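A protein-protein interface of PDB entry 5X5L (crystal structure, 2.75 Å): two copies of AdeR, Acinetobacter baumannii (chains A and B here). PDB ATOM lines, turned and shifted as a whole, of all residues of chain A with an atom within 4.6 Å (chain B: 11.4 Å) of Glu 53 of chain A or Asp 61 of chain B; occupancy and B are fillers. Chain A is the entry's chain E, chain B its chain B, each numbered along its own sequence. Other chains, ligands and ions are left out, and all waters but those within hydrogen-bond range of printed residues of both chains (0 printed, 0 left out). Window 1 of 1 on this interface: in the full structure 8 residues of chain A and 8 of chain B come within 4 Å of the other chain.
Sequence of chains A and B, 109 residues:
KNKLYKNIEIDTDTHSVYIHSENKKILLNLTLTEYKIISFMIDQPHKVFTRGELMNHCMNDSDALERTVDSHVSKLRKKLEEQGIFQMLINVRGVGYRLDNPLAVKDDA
Of the 12 printed residues of chain A, 6 touch a printed residue of chain B.
Along chain A the printed residues that touch a printed residue of chain B span positions 40 to 57.
Among the printed residues, 12 pairs touch across the chains.
The backbone NH (N) of Ser 62 of chain B sits at hydrogen-bond distance from the side-chain carboxylate (OE2) of Glu 53 of chain A (2.6 Å).
The side-chain carboxylate (OD2) of Asp 63 of chain B is in hydrogen-bond range of the backbone NH (N) of Glu 53 of chain A (3.1 Å).
The backbone NH of Asp 61 of chain B lies close to the side-chain carboxylate of Glu 53 of chain A (3.5 Å).
The backbone carbonyl oxygen (O) of Gly 52 of chain A lies close to the side-chain carboxylate (OD2) of Asp 63 of chain B, at 3.0 Å.
A ring nitrogen (NE2) of His 57 of chain A lies within hydrogen-bond range of the backbone carbonyl oxygen (O) of Ser 62 of chain B, 3.1 Å away.
The side-chain carboxylate of Asp 63 of chain B sits at hydrogen-bond distance from the side-chain amide nitrogen of Asn 56 of chain A, 3.5 Å away.
His 57 of chain A touches Asn 56 of chain B, but with the chains exchanged Asn 56 of chain A does not touch His 57 of chain B (13.5 Å).
Positions printed for both chains: 51, 52, 53, 54, 55, 56 and 57.
Of the 12 pairs that touch across the chains among the printed residues, none has its exchanged pair printed and touching as well.
Printed residues of chain B within 4 Å of Phe 40 of chain A: Asn 56 (3.2 Å) and Ser 62 (3.5 Å).
No residue of chain B comes within 4 Å of Phe 49 of chain A.
No residue of chain B comes within 4 Å of Thr 50 of chain A.
Gly 52 of chain A touches just one residue of chain B: Asp 63 (3.0 Å).
Of chain B, only Asp 61, Ser 62 and Asp 63 come within 4 Å of Glu 53 of chain A.
No residue of chain B comes within 4 Å of Leu 54 of chain A.
Printed residues of chain B within 4 Å of Asn 56 of chain A: Asp 63.
His 57 of chain A touches three residues of chain B.
Printed residues of chain A within 4 Å of Asn 56 of chain B: Phe 40 (3.2 Å) and His 57 (3.1 Å).
Asp 61 of chain B touches just one residue of chain A: Glu 53 (3.3 Å).
Printed residues of chain A within 4 Å of Ser 62 of chain B: Phe 40, Glu 53 and His 57.
The nearest residue of chain B that does not touch Glu 53 of chain A is Asn 60 of chain B (4.3 Å).
The nearest printed residue of chain A that does not touch Asp 61 of chain B is Lys 47 of chain A (4.6 Å).
The backbone carbonyl oxygen of Gly 52 of chain B lies close to the side-chain amide oxygen of Asn 56 of chain B, 3.3 Å away.
The backbone NH (N) of Thr 50 of chain A lies within hydrogen-bond range of the side-chain carboxylate (OE1) of Glu 53 of chain A, 3.0 Å away.
OD1 of Asp 61 of chain B sits close to N of Asp 63 of chain B.
N of Ala 64 of chain B sits at hydrogen-bond distance from OD1 of Asp 61 of chain B.
The backbone carbonyl oxygen (O) of Gly 52 of chain A lies close to the side-chain amide oxygen (OD1) of Asn 56 of chain A (3.3 Å).
The side-chain amino group (NZ) of Lys 47 of chain A lies within salt-bridge range of the side-chain carboxylate (OE1) of Glu 53 of chain A, at 2.9 Å.
Phe 40 of chain A touches Asn 56 of chain B (CE1 to ND2, 3.2 Å).
CZ of Phe 40 of chain A touches OG of Ser 62 of chain B, at 3.5 Å.
CE of Lys 47 of chain A touches O of Met 59 of chain B, 3.7 Å away.
Lys 47 of chain A touches Asn 60 of chain B.
OD1 of Asn 56 of chain B touches CE1 of His 57 of chain A, 3.1 Å away.
His 57 of chain A touches Asp 63 of chain B.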
ATOM      1  N   PHE A  40     -19.097  39.982   7.631  1.00  0.00           N
ATOM      2  CA  PHE A  40     -19.459  38.599   7.297  1.00  0.00           C
ATOM      3  C   PHE A  40     -18.965  38.226   5.907  1.00  0.00           C
ATOM      4  O   PHE A  40     -18.345  37.177   5.724  1.00  0.00           O
ATOM      5  CB  PHE A  40     -20.985  38.425   7.398  1.00  0.00           C
ATOM      6  CG  PHE A  40     -21.491  37.025   7.122  1.00  0.00           C
ATOM      7  CD1 PHE A  40     -20.835  35.897   7.617  1.00  0.00           C
ATOM      8  CD2 PHE A  40     -22.674  36.843   6.396  1.00  0.00           C
ATOM      9  CE1 PHE A  40     -21.309  34.634   7.335  1.00  0.00           C
ATOM     10  CE2 PHE A  40     -23.160  35.571   6.147  1.00  0.00           C
ATOM     11  CZ  PHE A  40     -22.474  34.463   6.627  1.00  0.00           C
ATOM     12  N   LYS A  47     -17.542  34.633  -2.548  1.00  0.00           N
ATOM     13  CA  LYS A  47     -18.707  33.776  -2.339  1.00  0.00           C
ATOM     14  C   LYS A  47     -20.011  34.537  -2.533  1.00  0.00           C
ATOM     15  O   LYS A  47     -20.128  35.696  -2.133  1.00  0.00           O
ATOM     16  CB  LYS A  47     -18.684  33.180  -0.934  1.00  0.00           C
ATOM     17  CG  LYS A  47     -19.808  32.197  -0.663  1.00  0.00           C
ATOM     18  CD  LYS A  47     -19.839  31.791   0.804  1.00  0.00           C
ATOM     19  CE  LYS A  47     -21.099  31.009   1.131  1.00  0.00           C
ATOM     20  NZ  LYS A  47     -22.267  31.860   1.379  1.00  0.00           N
ATOM     21  N   VAL A  48     -20.982  33.862  -3.137  1.00  0.00           N
ATOM     22  CA  VAL A  48     -22.355  34.355  -3.213  1.00  0.00           C
ATOM     23  C   VAL A  48     -23.066  33.943  -1.932  1.00  0.00           C
ATOM     24  O   VAL A  48     -23.245  32.748  -1.684  1.00  0.00           O
ATOM     25  CB  VAL A  48     -23.122  33.762  -4.422  1.00  0.00           C
ATOM     26  CG1 VAL A  48     -24.563  34.267  -4.444  1.00  0.00           C
ATOM     27  CG2 VAL A  48     -22.405  34.084  -5.719  1.00  0.00           C
ATOM     28  N   PHE A  49     -23.456  34.927  -1.129  1.00  0.00           N
ATOM     29  CA  PHE A  49     -24.271  34.687   0.063  1.00  0.00           C
ATOM     30  C   PHE A  49     -25.724  34.840  -0.315  1.00  0.00           C
ATOM     31  O   PHE A  49     -26.075  35.780  -1.017  1.00  0.00           O
ATOM     32  CB  PHE A  49     -23.916  35.684   1.165  1.00  0.00           C
ATOM     33  CG  PHE A  49     -22.522  35.516   1.684  1.00  0.00           C
ATOM     34  CD1 PHE A  49     -21.438  36.096   1.034  1.00  0.00           C
ATOM     35  CD2 PHE A  49     -22.287  34.743   2.803  1.00  0.00           C
ATOM     36  CE1 PHE A  49     -20.154  35.931   1.502  1.00  0.00           C
ATOM     37  CE2 PHE A  49     -20.995  34.566   3.285  1.00  0.00           C
ATOM     38  CZ  PHE A  49     -19.924  35.169   2.632  1.00  0.00           C
ATOM     39  N   THR A  50     -26.570  33.922   0.137  1.00  0.00           N
ATOM     40  CA  THR A  50     -28.010  34.042  -0.092  1.00  0.00           C
ATOM     41  C   THR A  50     -28.584  35.073   0.884  1.00  0.00           C
ATOM     42  O   THR A  50     -27.930  35.495   1.838  1.00  0.00           O
ATOM     43  CB  THR A  50     -28.753  32.699   0.104  1.00  0.00           C
ATOM     44  OG1 THR A  50     -28.531  32.193   1.430  1.00  0.00           O
ATOM     45  CG2 THR A  50     -28.253  31.654  -0.854  1.00  0.00           C
ATOM     46  N   ARG A  51     -29.815  35.481   0.622  1.00  0.00           N
ATOM     47  CA  ARG A  51     -30.522  36.412   1.495  1.00  0.00           C
ATOM     48  C   ARG A  51     -30.787  35.768   2.851  1.00  0.00           C
ATOM     49  O   ARG A  51     -30.697  36.438   3.874  1.00  0.00           O
ATOM     50  CB  ARG A  51     -31.824  36.892   0.848  1.00  0.00           C
ATOM     51  CG  ARG A  51     -31.584  37.750  -0.379  1.00  0.00           C
ATOM     52  CD  ARG A  51     -32.844  38.025  -1.167  1.00  0.00           C
ATOM     53  NE  ARG A  51     -32.676  39.107  -2.119  1.00  0.00           N
ATOM     54  CZ  ARG A  51     -32.125  39.010  -3.328  1.00  0.00           C
ATOM     55  NH1 ARG A  51     -31.663  37.853  -3.785  1.00  0.00           N
ATOM     56  NH2 ARG A  51     -32.030  40.097  -4.093  1.00  0.00           N
ATOM     57  N   GLY A  52     -31.097  34.475   2.847  1.00  0.00           N
ATOM     58  CA  GLY A  52     -31.283  33.704   4.074  1.00  0.00           C
ATOM     59  C   GLY A  52     -30.055  33.673   4.968  1.00  0.00           C
ATOM     60  O   GLY A  52     -30.179  33.762   6.198  1.00  0.00           O
ATOM     61  N   GLU A  53     -28.872  33.545   4.362  1.00  0.00           N
ATOM     62  CA  GLU A  53     -27.612  33.563   5.112  1.00  0.00           C
ATOM     63  C   GLU A  53     -27.321  34.927   5.707  1.00  0.00           C
ATOM     64  O   GLU A  53     -26.933  35.025   6.867  1.00  0.00           O
ATOM     65  CB  GLU A  53     -26.431  33.154   4.237  1.00  0.00           C
ATOM     66  CG  GLU A  53     -26.438  31.702   3.811  1.00  0.00           C
ATOM     67  CD  GLU A  53     -25.252  31.363   2.941  1.00  0.00           C
ATOM     68  OE1 GLU A  53     -25.103  31.950   1.853  1.00  0.00           O
ATOM     69  OE2 GLU A  53     -24.438  30.525   3.361  1.00  0.00           O
ATOM     70  N   LEU A  54     -27.501  35.977   4.911  1.00  0.00           N
ATOM     71  CA  LEU A  54     -27.303  37.350   5.384  1.00  0.00           C
ATOM     72  C   LEU A  54     -28.285  37.710   6.506  1.00  0.00           C
ATOM     73  O   LEU A  54     -27.898  38.372   7.468  1.00  0.00           O
ATOM     74  CB  LEU A  54     -27.420  38.345   4.231  1.00  0.00           C
ATOM     75  CG  LEU A  54     -26.329  38.236   3.157  1.00  0.00           C
ATOM     76  CD1 LEU A  54     -26.717  39.036   1.914  1.00  0.00           C
ATOM     77  CD2 LEU A  54     -24.981  38.692   3.694  1.00  0.00           C
ATOM     78  N   MET A  55     -29.526  37.246   6.389  1.00  0.00           N
ATOM     79  CA  MET A  55     -30.559  37.510   7.388  1.00  0.00           C
ATOM     80  C   MET A  55     -30.221  36.879   8.742  1.00  0.00           C
ATOM     81  O   MET A  55     -30.230  37.555   9.767  1.00  0.00           O
ATOM     82  CB  MET A  55     -31.927  36.990   6.908  1.00  0.00           C
ATOM     83  CG  MET A  55     -33.094  37.665   7.603  1.00  0.00           C
ATOM     84  SD  MET A  55     -34.671  37.381   6.850  1.00  0.00           S
ATOM     85  CE  MET A  55     -34.867  35.664   7.232  1.00  0.00           C
ATOM     86  N   ASN A  56     -29.909  35.587   8.727  1.00  0.00           N
ATOM     87  CA  ASN A  56     -29.580  34.845   9.949  1.00  0.00           C
ATOM     88  C   ASN A  56     -28.313  35.337  10.639  1.00  0.00           C
ATOM     89  O   ASN A  56     -28.210  35.272  11.858  1.00  0.00           O
ATOM     90  CB  ASN A  56     -29.432  33.343   9.648  1.00  0.00           C
ATOM     91  CG  ASN A  56     -30.746  32.675   9.308  1.00  0.00           C
ATOM     92  OD1 ASN A  56     -31.759  33.331   9.064  1.00  0.00           O
ATOM     93  ND2 ASN A  56     -30.737  31.352   9.299  1.00  0.00           N
ATOM     94  N   HIS A  57     -27.352  35.815   9.853  1.00  0.00           N
ATOM     95  CA  HIS A  57     -26.031  36.214  10.358  1.00  0.00           C
ATOM     96  C   HIS A  57     -25.918  37.699  10.690  1.00  0.00           C
ATOM     97  O   HIS A  57     -25.163  38.065  11.591  1.00  0.00           O
ATOM     98  CB  HIS A  57     -24.972  35.833   9.331  1.00  0.00           C
ATOM     99  CG  HIS A  57     -24.602  34.379   9.361  1.00  0.00           C
ATOM    100  ND1 HIS A  57     -23.572  33.922  10.135  1.00  0.00           N
ATOM    101  CD2 HIS A  57     -25.118  33.285   8.735  1.00  0.00           C
ATOM    102  CE1 HIS A  57     -23.447  32.613   9.978  1.00  0.00           C
ATOM    103  NE2 HIS A  57     -24.381  32.206   9.140  1.00  0.00           N
ATOM    104  N   LEU B  32     -12.624  21.389  -1.811  1.00  0.00           N
ATOM    105  CA  LEU B  32     -12.523  22.846  -1.677  1.00  0.00           C
ATOM    106  C   LEU B  32     -12.756  23.298  -0.235  1.00  0.00           C
ATOM    107  O   LEU B  32     -11.973  24.092   0.286  1.00  0.00           O
ATOM    108  CB  LEU B  32     -13.506  23.560  -2.602  1.00  0.00           C
ATOM    109  CG  LEU B  32     -13.423  25.093  -2.622  1.00  0.00           C
ATOM    110  CD1 LEU B  32     -12.061  25.584  -3.140  1.00  0.00           C
ATOM    111  CD2 LEU B  32     -14.577  25.677  -3.425  1.00  0.00           C
ATOM    112  N   THR B  33     -13.825  22.803   0.398  1.00  0.00           N
ATOM    113  CA  THR B  33     -14.076  23.084   1.814  1.00  0.00           C
ATOM    114  C   THR B  33     -12.877  22.700   2.677  1.00  0.00           C
ATOM    115  O   THR B  33     -12.400  23.502   3.472  1.00  0.00           O
ATOM    116  CB  THR B  33     -15.323  22.347   2.338  1.00  0.00           C
ATOM    117  OG1 THR B  33     -16.433  22.732   1.537  1.00  0.00           O
ATOM    118  CG2 THR B  33     -15.597  22.706   3.786  1.00  0.00           C
ATOM    119  N   LYS B  36      -9.953  25.043   2.284  1.00  0.00           N
ATOM    120  CA  LYS B  36     -10.192  26.308   2.978  1.00  0.00           C
ATOM    121  C   LYS B  36      -9.937  26.182   4.479  1.00  0.00           C
ATOM    122  O   LYS B  36      -9.319  27.058   5.075  1.00  0.00           O
ATOM    123  CB  LYS B  36     -11.613  26.823   2.719  1.00  0.00           C
ATOM    124  CG  LYS B  36     -11.829  27.363   1.315  1.00  0.00           C
ATOM    125  CD  LYS B  36     -13.147  28.117   1.196  1.00  0.00           C
ATOM    126  CE  LYS B  36     -13.590  28.252  -0.244  1.00  0.00           C
ATOM    127  NZ  LYS B  36     -12.893  29.374  -0.931  1.00  0.00           N
ATOM    128  N   ARG B  51     -16.787  26.826  15.597  1.00  0.00           N
ATOM    129  CA  ARG B  51     -17.491  26.239  14.462  1.00  0.00           C
ATOM    130  C   ARG B  51     -18.090  27.330  13.586  1.00  0.00           C
ATOM    131  O   ARG B  51     -18.093  27.208  12.364  1.00  0.00           O
ATOM    132  CB  ARG B  51     -18.581  25.271  14.940  1.00  0.00           C
ATOM    133  CG  ARG B  51     -18.008  24.035  15.588  1.00  0.00           C
ATOM    134  CD  ARG B  51     -19.069  23.214  16.313  1.00  0.00           C
ATOM    135  NE  ARG B  51     -18.583  21.889  16.664  1.00  0.00           N
ATOM    136  CZ  ARG B  51     -17.809  21.589  17.714  1.00  0.00           C
ATOM    137  NH1 ARG B  51     -17.369  22.530  18.560  1.00  0.00           N
ATOM    138  NH2 ARG B  51     -17.431  20.326  17.905  1.00  0.00           N
ATOM    139  N   GLY B  52     -18.586  28.395  14.219  1.00  0.00           N
ATOM    140  CA  GLY B  52     -19.098  29.563  13.500  1.00  0.00           C
ATOM    141  C   GLY B  52     -18.069  30.239  12.615  1.00  0.00           C
ATOM    142  O   GLY B  52     -18.395  30.660  11.519  1.00  0.00           O
ATOM    143  N   GLU B  53     -16.831  30.341  13.091  1.00  0.00           N
ATOM    144  CA  GLU B  53     -15.737  30.929  12.302  1.00  0.00           C
ATOM    145  C   GLU B  53     -15.365  30.052  11.115  1.00  0.00           C
ATOM    146  O   GLU B  53     -15.180  30.556  10.014  1.00  0.00           O
ATOM    147  CB  GLU B  53     -14.489  31.161  13.151  1.00  0.00           C
ATOM    148  CG  GLU B  53     -14.638  32.239  14.188  1.00  0.00           C
ATOM    149  CD  GLU B  53     -13.395  32.417  15.026  1.00  0.00           C
ATOM    150  OE1 GLU B  53     -12.915  31.436  15.651  1.00  0.00           O
ATOM    151  OE2 GLU B  53     -12.979  33.568  15.098  1.00  0.00           O
ATOM    152  N   LEU B  54     -15.242  28.748  11.350  1.00  0.00           N
ATOM    153  CA  LEU B  54     -14.943  27.801  10.275  1.00  0.00           C
ATOM    154  C   LEU B  54     -16.055  27.764   9.216  1.00  0.00           C
ATOM    155  O   LEU B  54     -15.773  27.683   8.031  1.00  0.00           O
ATOM    156  CB  LEU B  54     -14.701  26.400  10.843  1.00  0.00           C
ATOM    157  CG  LEU B  54     -13.465  26.257  11.733  1.00  0.00           C
ATOM    158  CD1 LEU B  54     -13.504  24.936  12.490  1.00  0.00           C
ATOM    159  CD2 LEU B  54     -12.185  26.371  10.919  1.00  0.00           C
ATOM    160  N   MET B  55     -17.306  27.851   9.655  1.00  0.00           N
ATOM    161  CA  MET B  55     -18.464  27.835   8.753  1.00  0.00           C
ATOM    162  C   MET B  55     -18.478  29.060   7.836  1.00  0.00           C
ATOM    163  O   MET B  55     -18.585  28.925   6.622  1.00  0.00           O
ATOM    164  CB  MET B  55     -19.772  27.784   9.552  1.00  0.00           C
ATOM    165  CG  MET B  55     -20.942  27.247   8.740  1.00  0.00           C
ATOM    166  SD  MET B  55     -22.539  26.914   9.538  1.00  0.00           S
ATOM    167  CE  MET B  55     -22.066  26.118  11.074  1.00  0.00           C
ATOM    168  N   ASN B  56     -18.351  30.246   8.422  1.00  0.00           N
ATOM    169  CA  ASN B  56     -18.360  31.503   7.666  1.00  0.00           C
ATOM    170  C   ASN B  56     -17.184  31.638   6.694  1.00  0.00           C
ATOM    171  O   ASN B  56     -17.325  32.250   5.638  1.00  0.00           O
ATOM    172  CB  ASN B  56     -18.354  32.716   8.615  1.00  0.00           C
ATOM    173  CG  ASN B  56     -19.647  32.874   9.388  1.00  0.00           C
ATOM    174  OD1 ASN B  56     -20.510  31.987   9.393  1.00  0.00           O
ATOM    175  ND2 ASN B  56     -19.797  34.027  10.034  1.00  0.00           N
ATOM    176  N   HIS B  57     -16.038  31.074   7.059  1.00  0.00           N
ATOM    177  CA  HIS B  57     -14.802  31.215   6.291  1.00  0.00           C
ATOM    178  C   HIS B  57     -14.551  30.085   5.287  1.00  0.00           C
ATOM    179  O   HIS B  57     -13.934  30.314   4.250  1.00  0.00           O
ATOM    180  CB  HIS B  57     -13.622  31.316   7.257  1.00  0.00           C
ATOM    181  CG  HIS B  57     -13.443  32.676   7.843  1.00  0.00           C
ATOM    182  ND1 HIS B  57     -14.161  33.141   8.929  1.00  0.00           N
ATOM    183  CD2 HIS B  57     -12.618  33.682   7.478  1.00  0.00           C
ATOM    184  CE1 HIS B  57     -13.772  34.371   9.211  1.00  0.00           C
ATOM    185  NE2 HIS B  57     -12.842  34.726   8.340  1.00  0.00           N
ATOM    186  N   CYS B  58     -15.016  28.877   5.592  1.00  0.00           N
ATOM    187  CA  CYS B  58     -14.640  27.689   4.823  1.00  0.00           C
ATOM    188  C   CYS B  58     -15.766  26.905   4.135  1.00  0.00           C
ATOM    189  O   CYS B  58     -15.468  25.976   3.384  1.00  0.00           O
ATOM    190  CB  CYS B  58     -13.853  26.733   5.723  1.00  0.00           C
ATOM    191  SG  CYS B  58     -12.543  27.544   6.657  1.00  0.00           S
ATOM    192  N   MET B  59     -17.028  27.278   4.338  1.00  0.00           N
ATOM    193  CA  MET B  59     -18.155  26.519   3.789  1.00  0.00           C
ATOM    194  C   MET B  59     -19.074  27.359   2.893  1.00  0.00           C
ATOM    195  O   MET B  59     -19.072  28.589   2.987  1.00  0.00           O
ATOM    196  CB  MET B  59     -18.966  25.913   4.939  1.00  0.00           C
ATOM    197  CG  MET B  59     -18.217  24.826   5.692  1.00  0.00           C
ATOM    198  SD  MET B  59     -19.064  24.192   7.175  1.00  0.00           S
ATOM    199  CE  MET B  59     -20.788  24.127   6.683  1.00  0.00           C
ATOM    200  N   ASN B  60     -19.886  26.695   2.060  1.00  0.00           N
ATOM    201  CA  ASN B  60     -21.176  27.262   1.598  1.00  0.00           C
ATOM    202  C   ASN B  60     -22.211  26.951   2.696  1.00  0.00           C
ATOM    203  O   ASN B  60     -21.885  26.389   3.755  1.00  0.00           O
ATOM    204  CB  ASN B  60     -21.583  26.708   0.225  1.00  0.00           C
ATOM    205  CG  ASN B  60     -20.484  26.841  -0.813  1.00  0.00           C
ATOM    206  OD1 ASN B  60     -19.285  26.684  -0.520  1.00  0.00           O
ATOM    207  ND2 ASN B  60     -20.889  27.107  -2.052  1.00  0.00           N
ATOM    208  N   ASP B  61     -23.450  27.332   2.476  1.00  0.00           N
ATOM    209  CA  ASP B  61     -24.464  27.235   3.512  1.00  0.00           C
ATOM    210  C   ASP B  61     -23.943  27.517   4.937  1.00  0.00           C
ATOM    211  O   ASP B  61     -23.805  26.627   5.772  1.00  0.00           O
ATOM    212  CB  ASP B  61     -25.207  25.900   3.439  1.00  0.00           C
ATOM    213  CG  ASP B  61     -26.630  26.001   3.986  1.00  0.00           C
ATOM    214  OD1 ASP B  61     -27.090  27.137   4.233  1.00  0.00           O
ATOM    215  OD2 ASP B  61     -27.308  24.958   4.161  1.00  0.00           O
ATOM    216  N   SER B  62     -23.637  28.787   5.169  1.00  0.00           N
ATOM    217  CA  SER B  62     -23.509  29.365   6.501  1.00  0.00           C
ATOM    218  C   SER B  62     -24.755  29.140   7.376  1.00  0.00           C
ATOM    219  O   SER B  62     -24.661  29.123   8.613  1.00  0.00           O
ATOM    220  CB  SER B  62     -23.260  30.866   6.361  1.00  0.00           C
ATOM    221  OG  SER B  62     -22.144  31.155   5.503  1.00  0.00           O
ATOM    222  N   ASP B  63     -25.915  28.981   6.724  1.00  0.00           N
ATOM    223  CA  ASP B  63     -27.134  28.438   7.377  1.00  0.00           C
ATOM    224  C   ASP B  63     -27.168  26.946   7.654  1.00  0.00           C
ATOM    225  O   ASP B  63     -28.190  26.478   8.174  1.00  0.00           O
ATOM    226  CB  ASP B  63     -28.413  28.903   6.622  1.00  0.00           C
ATOM    227  CG  ASP B  63     -28.558  30.382   6.587  1.00  0.00           C
ATOM    228  OD1 ASP B  63     -27.880  31.115   7.337  1.00  0.00           O
ATOM    229  OD2 ASP B  63     -29.381  30.849   5.785  1.00  0.00           O
ATOM    230  N   ALA B  64     -26.083  26.202   7.401  1.00  0.00           N
ATOM    231  CA  ALA B  64     -26.033  24.782   7.730  1.00  0.00           C
ATOM    232  C   ALA B  64     -25.838  24.586   9.234  1.00  0.00           C
ATOM    233  O   ALA B  64     -25.684  25.574   9.998  1.00  0.00           O
ATOM    234  CB  ALA B  64     -24.920  24.073   6.968  1.00  0.00           C
ATOM    235  N   LEU B  65     -25.914  23.332   9.668  1.00  0.00           N
ATOM    236  CA  LEU B  65     -25.687  22.997  11.082  1.00  0.00           C
ATOM    237  C   LEU B  65     -24.223  23.112  11.459  1.00  0.00           C
ATOM    238  O   LEU B  65     -23.351  22.911  10.621  1.00  0.00           O
ATOM    239  CB  LEU B  65     -26.157  21.571  11.383  1.00  0.00           C
ATOM    240  CG  LEU B  65     -27.637  21.239  11.113  1.00  0.00           C
ATOM    241  CD1 LEU B  65     -27.919  19.747  11.272  1.00  0.00           C
ATOM    242  CD2 LEU B  65     -28.584  22.055  11.989  1.00  0.00           C
ATOM    243  N   GLU B  66     -23.951  23.367  12.735  1.00  0.00           N
ATOM    244  CA  GLU B  66     -22.571  23.417  13.227  1.00  0.00           C
ATOM    245  C   GLU B  66     -21.933  22.031  13.235  1.00  0.00           C
ATOM    246  O   GLU B  66     -20.723  21.897  13.083  1.00  0.00           O
ATOM    247  CB  GLU B  66     -22.496  24.072  14.606  1.00  0.00           C
ATOM    248  CG  GLU B  66     -22.757  25.583  14.539  1.00  0.00           C
ATOM    249  CD  GLU B  66     -22.612  26.297  15.865  1.00  0.00           C
ATOM    250  OE1 GLU B  66     -23.118  25.749  16.871  1.00  0.00           O
ATOM    251  OE2 GLU B  66     -22.012  27.413  15.892  1.00  0.00           O
ATOM    252  N   ARG B  67     -22.746  20.996  13.387  1.00  0.00           N
ATOM    253  CA  ARG B  67     -22.239  19.628  13.318  1.00  0.00           C
ATOM    254  C   ARG B  67     -21.630  19.295  11.956  1.00  0.00           C
ATOM    255  O   ARG B  67     -20.699  18.518  11.879  1.00  0.00           O
ATOM    256  CB  ARG B  67     -23.289  18.611  13.735  1.00  0.00           C
ATOM    257  CG  ARG B  67     -23.701  18.734  15.203  1.00  0.00           C
ATOM    258  CD  ARG B  67     -22.621  18.313  16.179  1.00  0.00           C
ATOM    259  NE  ARG B  67     -22.838  18.933  17.489  1.00  0.00           N
ATOM    260  CZ  ARG B  67     -21.889  19.287  18.360  1.00  0.00           C
ATOM    261  NH1 ARG B  67     -20.587  19.131  18.098  1.00  0.00           N
ATOM    262  NH2 ARG B  67     -22.247  19.820  19.532  1.00  0.00           N
ATOM    263  N   THR B  68     -22.138  19.893  10.887  1.00  0.00           N
ATOM    264  CA  THR B  68     -21.561  19.718   9.536  1.00  0.00           C
ATOM    265  C   THR B  68     -20.119  20.206   9.446  1.00  0.00           C
ATOM    266  O   THR B  68     -19.335  19.640   8.722  1.00  0.00           O
ATOM    267  CB  THR B  68     -22.438  20.406   8.462  1.00  0.00           C
ATOM    268  OG1 THR B  68     -23.705  19.746   8.411  1.00  0.00           O
ATOM    269  CG2 THR B  68     -21.811  20.354   7.085  1.00  0.00           C
ATOM    270  N   VAL B  69     -19.782  21.266  10.161  1.00  0.00           N
ATOM    271  CA  VAL B  69     -18.380  21.675  10.361  1.00  0.00           C
ATOM    272  C   VAL B  69     -17.542  20.515  10.895  1.00  0.00           C
ATOM    273  O   VAL B  69     -16.479  20.261  10.369  1.00  0.00           O
ATOM    274  CB  VAL B  69     -18.219  22.831  11.391  1.00  0.00           C
ATOM    275  CG1 VAL B  69     -16.755  23.256  11.485  1.00  0.00           C
ATOM    276  CG2 VAL B  69     -19.111  24.021  11.041  1.00  0.00           C
ATOM    277  N   ASP B  70     -18.032  19.832  11.926  1.00  0.00           N
ATOM    278  CA  ASP B  70     -17.320  18.701  12.536  1.00  0.00           C
ATOM    279  C   ASP B  70     -16.986  17.644  11.478  1.00  0.00           C
ATOM    280  O   ASP B  70     -15.866  17.135  11.432  1.00  0.00           O
ATOM    281  CB  ASP B  70     -18.122  18.025  13.671  1.00  0.00           C
ATOM    282  CG  ASP B  70     -18.548  18.989  14.787  1.00  0.00           C
ATOM    283  OD1 ASP B  70     -18.348  20.212  14.645  1.00  0.00           O
ATOM    284  OD2 ASP B  70     -19.074  18.507  15.815  1.00  0.00           O
ATOM    285  N   HIS B  72     -16.680  17.992   8.153  1.00  0.00           N
ATOM    286  CA  HIS B  72     -15.621  18.455   7.242  1.00  0.00           C
ATOM    287  C   HIS B  72     -14.252  18.325   7.878  1.00  0.00           C
ATOM    288  O   HIS B  72     -13.300  17.957   7.196  1.00  0.00           O
ATOM    289  CB  HIS B  72     -15.820  19.906   6.775  1.00  0.00           C
ATOM    290  CG  HIS B  72     -16.905  20.076   5.760  1.00  0.00           C
ATOM    291  ND1 HIS B  72     -16.764  19.688   4.446  1.00  0.00           N
ATOM    292  CD2 HIS B  72     -18.136  20.622   5.862  1.00  0.00           C
ATOM    293  CE1 HIS B  72     -17.879  19.957   3.790  1.00  0.00           C
ATOM    294  NE2 HIS B  72     -18.725  20.533   4.625  1.00  0.00           N
